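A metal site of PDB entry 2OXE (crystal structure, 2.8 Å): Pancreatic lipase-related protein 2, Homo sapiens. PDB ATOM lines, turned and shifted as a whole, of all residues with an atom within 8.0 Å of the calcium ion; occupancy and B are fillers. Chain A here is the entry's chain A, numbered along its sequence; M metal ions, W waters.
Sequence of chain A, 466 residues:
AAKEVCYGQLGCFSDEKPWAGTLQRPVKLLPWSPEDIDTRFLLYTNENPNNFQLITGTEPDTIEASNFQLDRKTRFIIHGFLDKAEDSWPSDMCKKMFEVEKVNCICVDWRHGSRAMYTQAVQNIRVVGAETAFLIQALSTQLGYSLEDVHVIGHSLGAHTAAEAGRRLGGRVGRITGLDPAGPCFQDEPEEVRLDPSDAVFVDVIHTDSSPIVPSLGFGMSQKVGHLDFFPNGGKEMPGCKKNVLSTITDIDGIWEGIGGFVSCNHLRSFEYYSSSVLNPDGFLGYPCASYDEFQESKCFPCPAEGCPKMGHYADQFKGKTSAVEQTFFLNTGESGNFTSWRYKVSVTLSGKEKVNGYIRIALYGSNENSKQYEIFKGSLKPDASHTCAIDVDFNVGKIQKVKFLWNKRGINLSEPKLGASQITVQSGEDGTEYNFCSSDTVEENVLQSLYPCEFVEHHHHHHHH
The side-chain hydroxyl (OG) of Ser 198 is in hydrogen-bond range of the side-chain carboxylate (OD1) of Asp 196, at 2.7 Å.
Four residues have an atom within 4 Å of the calcium ion: Glu 191, Arg 194, Asp 196 and Asp 199.
The nearest printed residue that does not touch the calcium ion is Glu 192 (4.3 Å).
OD2 of Asp 196 binds the calcium ion (2.3 Å).
The calcium ion is bound by the backbone carbonyl oxygen (O) of Arg 194 (2.4 Å).
The calcium ion is bound by O of Glu 191 (2.4 Å).
The side-chain carboxylate (OD1) of Asp 199 binds the calcium ion (2.7 Å).
The calcium ion is bound by the side-chain carboxylate (OD2) of Asp 199 (2.7 Å).
Water W1 is bound to the calcium ion, at 2.7 Å.
The calcium ion has six donor atoms within binding distance.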
ATOM      1  N   TRP A  19      11.808 -24.528  -3.906  1.00  0.00           N
ATOM      2  CA  TRP A  19      10.732 -23.548  -3.748  1.00  0.00           C
ATOM      3  C   TRP A  19       9.493 -23.890  -4.563  1.00  0.00           C
ATOM      4  O   TRP A  19       8.372 -23.646  -4.111  1.00  0.00           O
ATOM      5  CB  TRP A  19      11.218 -22.127  -4.055  1.00  0.00           C
ATOM      6  CG  TRP A  19      12.374 -21.722  -3.188  1.00  0.00           C
ATOM      7  CD1 TRP A  19      13.672 -21.575  -3.584  1.00  0.00           C
ATOM      8  CD2 TRP A  19      12.335 -21.467  -1.788  1.00  0.00           C
ATOM      9  NE1 TRP A  19      14.446 -21.214  -2.515  1.00  0.00           N
ATOM     10  CE2 TRP A  19      13.655 -21.131  -1.392  1.00  0.00           C
ATOM     11  CE3 TRP A  19      11.327 -21.461  -0.818  1.00  0.00           C
ATOM     12  CZ2 TRP A  19      13.993 -20.808  -0.074  1.00  0.00           C
ATOM     13  CZ3 TRP A  19      11.665 -21.154   0.483  1.00  0.00           C
ATOM     14  CH2 TRP A  19      12.980 -20.830   0.842  1.00  0.00           C
ATOM     15  N   ALA A 159       4.349 -20.562  11.264  1.00  0.00           N
ATOM     16  CA  ALA A 159       5.518 -21.300  11.747  1.00  0.00           C
ATOM     17  C   ALA A 159       6.628 -21.385  10.696  1.00  0.00           C
ATOM     18  O   ALA A 159       7.808 -21.283  11.035  1.00  0.00           O
ATOM     19  CB  ALA A 159       5.115 -22.686  12.224  1.00  0.00           C
ATOM     20  N   HIS A 160       6.268 -21.569   9.431  1.00  0.00           N
ATOM     21  CA  HIS A 160       7.286 -21.661   8.382  1.00  0.00           C
ATOM     22  C   HIS A 160       7.763 -20.282   7.974  1.00  0.00           C
ATOM     23  O   HIS A 160       8.880 -20.128   7.468  1.00  0.00           O
ATOM     24  CB  HIS A 160       6.752 -22.422   7.174  1.00  0.00           C
ATOM     25  CG  HIS A 160       6.251 -23.789   7.496  1.00  0.00           C
ATOM     26  ND1 HIS A 160       7.069 -24.786   7.973  1.00  0.00           N
ATOM     27  CD2 HIS A 160       5.015 -24.315   7.405  1.00  0.00           C
ATOM     28  CE1 HIS A 160       6.356 -25.881   8.167  1.00  0.00           C
ATOM     29  NE2 HIS A 160       5.103 -25.625   7.827  1.00  0.00           N
ATOM     30  N   ALA A 162       8.012 -17.865  10.348  1.00  0.00           N
ATOM     31  CA  ALA A 162       8.982 -17.853  11.435  1.00  0.00           C
ATOM     32  C   ALA A 162      10.292 -18.482  10.992  1.00  0.00           C
ATOM     33  O   ALA A 162      11.329 -17.829  11.031  1.00  0.00           O
ATOM     34  CB  ALA A 162       8.429 -18.606  12.664  1.00  0.00           C
ATOM     35  N   ALA A 163      10.209 -19.738  10.538  1.00  0.00           N
ATOM     36  CA  ALA A 163      11.358 -20.540  10.083  1.00  0.00           C
ATOM     37  C   ALA A 163      12.204 -19.845   9.042  1.00  0.00           C
ATOM     38  O   ALA A 163      13.436 -19.875   9.122  1.00  0.00           O
ATOM     39  CB  ALA A 163      10.870 -21.846   9.540  1.00  0.00           C
ATOM     40  N   GLU A 164      11.538 -19.239   8.052  1.00  0.00           N
ATOM     41  CA  GLU A 164      12.181 -18.504   6.988  1.00  0.00           C
ATOM     42  C   GLU A 164      13.008 -17.355   7.535  1.00  0.00           C
ATOM     43  O   GLU A 164      14.164 -17.184   7.167  1.00  0.00           O
ATOM     44  CB  GLU A 164      11.129 -17.980   6.002  1.00  0.00           C
ATOM     45  CG  GLU A 164      11.680 -17.282   4.770  1.00  0.00           C
ATOM     46  CD  GLU A 164      12.406 -18.228   3.815  1.00  0.00           C
ATOM     47  OE1 GLU A 164      12.936 -17.721   2.804  1.00  0.00           O
ATOM     48  OE2 GLU A 164      12.437 -19.461   4.070  1.00  0.00           O
ATOM     49  N   ALA A 165      12.416 -16.551   8.426  1.00  0.00           N
ATOM     50  CA  ALA A 165      13.153 -15.469   9.057  1.00  0.00           C
ATOM     51  C   ALA A 165      14.351 -16.030   9.828  1.00  0.00           C
ATOM     52  O   ALA A 165      15.440 -15.463   9.794  1.00  0.00           O
ATOM     53  CB  ALA A 165      12.238 -14.678   9.966  1.00  0.00           C
ATOM     54  N   GLY A 166      14.156 -17.172  10.490  1.00  0.00           N
ATOM     55  CA  GLY A 166      15.220 -17.831  11.232  1.00  0.00           C
ATOM     56  C   GLY A 166      16.391 -18.220  10.368  1.00  0.00           C
ATOM     57  O   GLY A 166      17.549 -17.952  10.708  1.00  0.00           O
ATOM     58  N   ARG A 167      16.097 -18.859   9.242  1.00  0.00           N
ATOM     59  CA  ARG A 167      17.106 -19.135   8.221  1.00  0.00           C
ATOM     60  C   ARG A 167      17.809 -17.854   7.736  1.00  0.00           C
ATOM     61  O   ARG A 167      19.032 -17.776   7.792  1.00  0.00           O
ATOM     62  CB  ARG A 167      16.479 -19.862   7.043  1.00  0.00           C
ATOM     63  CG  ARG A 167      17.501 -20.294   6.029  1.00  0.00           C
ATOM     64  CD  ARG A 167      16.818 -20.962   4.870  1.00  0.00           C
ATOM     65  NE  ARG A 167      15.952 -20.041   4.138  1.00  0.00           N
ATOM     66  CZ  ARG A 167      16.395 -19.182   3.224  1.00  0.00           C
ATOM     67  NH1 ARG A 167      15.543 -18.383   2.604  1.00  0.00           N
ATOM     68  NH2 ARG A 167      17.702 -19.129   2.932  1.00  0.00           N
ATOM     69  N   ARG A 168      17.037 -16.876   7.271  1.00  0.00           N
ATOM     70  CA  ARG A 168      17.585 -15.568   6.867  1.00  0.00           C
ATOM     71  C   ARG A 168      18.592 -14.968   7.877  1.00  0.00           C
ATOM     72  O   ARG A 168      19.473 -14.189   7.481  1.00  0.00           O
ATOM     73  CB  ARG A 168      16.462 -14.565   6.601  1.00  0.00           C
ATOM     74  CG  ARG A 168      16.056 -14.411   5.148  1.00  0.00           C
ATOM     75  CD  ARG A 168      15.082 -15.490   4.711  1.00  0.00           C
ATOM     76  NE  ARG A 168      14.502 -15.293   3.368  1.00  0.00           N
ATOM     77  CZ  ARG A 168      14.741 -14.251   2.555  1.00  0.00           C
ATOM     78  NH1 ARG A 168      14.148 -14.208   1.379  1.00  0.00           N
ATOM     79  NH2 ARG A 168      15.543 -13.257   2.921  1.00  0.00           N
ATOM     80  N   ILE A 176      12.232 -20.118  18.268  1.00  0.00           N
ATOM     81  CA  ILE A 176      11.040 -20.232  17.438  1.00  0.00           C
ATOM     82  C   ILE A 176      10.068 -21.249  18.015  1.00  0.00           C
ATOM     83  O   ILE A 176      10.469 -22.334  18.427  1.00  0.00           O
ATOM     84  CB  ILE A 176      11.328 -20.587  15.970  1.00  0.00           C
ATOM     85  CG1 ILE A 176      11.923 -19.378  15.244  1.00  0.00           C
ATOM     86  CG2 ILE A 176      10.044 -20.983  15.283  1.00  0.00           C
ATOM     87  CD1 ILE A 176      12.276 -19.616  13.774  1.00  0.00           C
ATOM     88  N   PRO A 190      12.561 -30.418   1.969  1.00  0.00           N
ATOM     89  CA  PRO A 190      13.895 -30.112   2.501  1.00  0.00           C
ATOM     90  C   PRO A 190      13.850 -28.964   3.488  1.00  0.00           C
ATOM     91  O   PRO A 190      12.987 -28.106   3.388  1.00  0.00           O
ATOM     92  CB  PRO A 190      14.686 -29.680   1.254  1.00  0.00           C
ATOM     93  CG  PRO A 190      13.883 -30.072   0.103  1.00  0.00           C
ATOM     94  CD  PRO A 190      12.466 -30.045   0.551  1.00  0.00           C
ATOM     95  N   GLU A 191      14.815 -28.951   4.406  1.00  0.00           N
ATOM     96  CA  GLU A 191      14.893 -27.981   5.500  1.00  0.00           C
ATOM     97  C   GLU A 191      14.887 -26.513   5.093  1.00  0.00           C
ATOM     98  O   GLU A 191      14.550 -25.655   5.898  1.00  0.00           O
ATOM     99  CB  GLU A 191      16.117 -28.278   6.353  1.00  0.00           C
ATOM    100  CG  GLU A 191      15.905 -29.494   7.241  1.00  0.00           C
ATOM    101  CD  GLU A 191      17.192 -30.185   7.664  1.00  0.00           C
ATOM    102  OE1 GLU A 191      18.211 -30.086   6.934  1.00  0.00           O
ATOM    103  OE2 GLU A 191      17.173 -30.856   8.726  1.00  0.00           O
ATOM    104  N   GLU A 192      15.261 -26.234   3.845  1.00  0.00           N
ATOM    105  CA  GLU A 192      15.346 -24.878   3.327  1.00  0.00           C
ATOM    106  C   GLU A 192      13.993 -24.196   3.335  1.00  0.00           C
ATOM    107  O   GLU A 192      13.893 -22.984   3.548  1.00  0.00           O
ATOM    108  CB  GLU A 192      15.896 -24.885   1.899  1.00  0.00           C
ATOM    109  CG  GLU A 192      16.189 -23.507   1.288  1.00  0.00           C
ATOM    110  CD  GLU A 192      17.574 -22.959   1.641  1.00  0.00           C
ATOM    111  OE1 GLU A 192      18.377 -23.704   2.260  1.00  0.00           O
ATOM    112  OE2 GLU A 192      17.856 -21.786   1.309  1.00  0.00           O
ATOM    113  N   VAL A 193      12.938 -24.984   3.109  1.00  0.00           N
ATOM    114  CA  VAL A 193      11.621 -24.408   2.852  1.00  0.00           C
ATOM    115  C   VAL A 193      10.664 -24.544   4.021  1.00  0.00           C
ATOM    116  O   VAL A 193       9.576 -23.959   4.001  1.00  0.00           O
ATOM    117  CB  VAL A 193      10.984 -24.970   1.559  1.00  0.00           C
ATOM    118  CG1 VAL A 193      11.983 -24.883   0.412  1.00  0.00           C
ATOM    119  CG2 VAL A 193      10.505 -26.400   1.762  1.00  0.00           C
ATOM    120  N   ARG A 194      11.057 -25.287   5.041  1.00  0.00           N
ATOM    121  CA  ARG A 194      10.194 -25.528   6.192  1.00  0.00           C
ATOM    122  C   ARG A 194      10.847 -25.185   7.522  1.00  0.00           C
ATOM    123  O   ARG A 194      12.045 -24.855   7.585  1.00  0.00           O
ATOM    124  CB  ARG A 194       9.708 -26.976   6.201  1.00  0.00           C
ATOM    125  CG  ARG A 194      10.832 -27.987   6.333  1.00  0.00           C
ATOM    126  CD  ARG A 194      10.282 -29.329   6.695  1.00  0.00           C
ATOM    127  NE  ARG A 194      11.314 -30.367   6.655  1.00  0.00           N
ATOM    128  CZ  ARG A 194      12.089 -30.697   7.682  1.00  0.00           C
ATOM    129  NH1 ARG A 194      12.976 -31.682   7.556  1.00  0.00           N
ATOM    130  NH2 ARG A 194      11.960 -30.064   8.844  1.00  0.00           N
ATOM    131  N   LEU A 195      10.061 -25.279   8.585  1.00  0.00           N
ATOM    132  CA  LEU A 195      10.614 -25.154   9.922  1.00  0.00           C
ATOM    133  C   LEU A 195      11.466 -26.398  10.189  1.00  0.00           C
ATOM    134  O   LEU A 195      11.120 -27.506   9.758  1.00  0.00           O
ATOM    135  CB  LEU A 195       9.504 -24.995  10.970  1.00  0.00           C
ATOM    136  CG  LEU A 195       9.909 -24.895  12.457  1.00  0.00           C
ATOM    137  CD1 LEU A 195      10.806 -23.686  12.703  1.00  0.00           C
ATOM    138  CD2 LEU A 195       8.696 -24.855  13.386  1.00  0.00           C
ATOM    139  N   ASP A 196      12.600 -26.198  10.849  1.00  0.00           N
ATOM    140  CA  ASP A 196      13.457 -27.294  11.290  1.00  0.00           C
ATOM    141  C   ASP A 196      14.364 -26.761  12.385  1.00  0.00           C
ATOM    142  O   ASP A 196      14.562 -25.549  12.481  1.00  0.00           O
ATOM    143  CB  ASP A 196      14.253 -27.889  10.120  1.00  0.00           C
ATOM    144  CG  ASP A 196      15.288 -26.939   9.558  1.00  0.00           C
ATOM    145  OD1 ASP A 196      16.492 -27.244   9.729  1.00  0.00           O
ATOM    146  OD2 ASP A 196      14.905 -25.913   8.941  1.00  0.00           O
ATOM    147  N   PRO A 197      14.908 -27.664  13.240  1.00  0.00           N
ATOM    148  CA  PRO A 197      15.729 -27.305  14.410  1.00  0.00           C
ATOM    149  C   PRO A 197      16.842 -26.266  14.170  1.00  0.00           C
ATOM    150  O   PRO A 197      17.243 -25.578  15.110  1.00  0.00           O
ATOM    151  CB  PRO A 197      16.358 -28.639  14.804  1.00  0.00           C
ATOM    152  CG  PRO A 197      15.365 -29.642  14.386  1.00  0.00           C
ATOM    153  CD  PRO A 197      14.733 -29.119  13.134  1.00  0.00           C
ATOM    154  N   SER A 198      17.310 -26.150  12.922  1.00  0.00           N
ATOM    155  CA  SER A 198      18.447 -25.271  12.625  1.00  0.00           C
ATOM    156  C   SER A 198      18.064 -23.800  12.500  1.00  0.00           C
ATOM    157  O   SER A 198      18.928 -22.930  12.414  1.00  0.00           O
ATOM    158  CB  SER A 198      19.217 -25.753  11.389  1.00  0.00           C
ATOM    159  OG  SER A 198      18.500 -25.518  10.186  1.00  0.00           O
ATOM    160  N   ASP A 199      16.760 -23.521  12.516  1.00  0.00           N
ATOM    161  CA  ASP A 199      16.223 -22.182  12.259  1.00  0.00           C
ATOM    162  C   ASP A 199      16.385 -21.185  13.389  1.00  0.00           C
ATOM    163  O   ASP A 199      16.334 -19.972  13.185  1.00  0.00           O
ATOM    164  CB  ASP A 199      14.747 -22.269  11.873  1.00  0.00           C
ATOM    165  CG  ASP A 199      14.565 -22.814  10.495  1.00  0.00           C
ATOM    166  OD1 ASP A 199      15.447 -22.596   9.645  1.00  0.00           O
ATOM    167  OD2 ASP A 199      13.537 -23.466  10.243  1.00  0.00           O
ATOM    168  N   ALA A 200      16.591 -21.708  14.591  1.00  0.00           N
ATOM    169  CA  ALA A 200      16.770 -20.866  15.759  1.00  0.00           C
ATOM    170  C   ALA A 200      17.578 -21.664  16.763  1.00  0.00           C
ATOM    171  O   ALA A 200      17.701 -22.878  16.633  1.00  0.00           O
ATOM    172  CB  ALA A 200      15.423 -20.467  16.343  1.00  0.00           C
HETATM  173 CA    CA M   1      14.274 -24.027   7.706  1.00  0.00          CA
HETATM  174  O   HOH W   1      13.148 -21.894   6.401  1.00  0.00           O
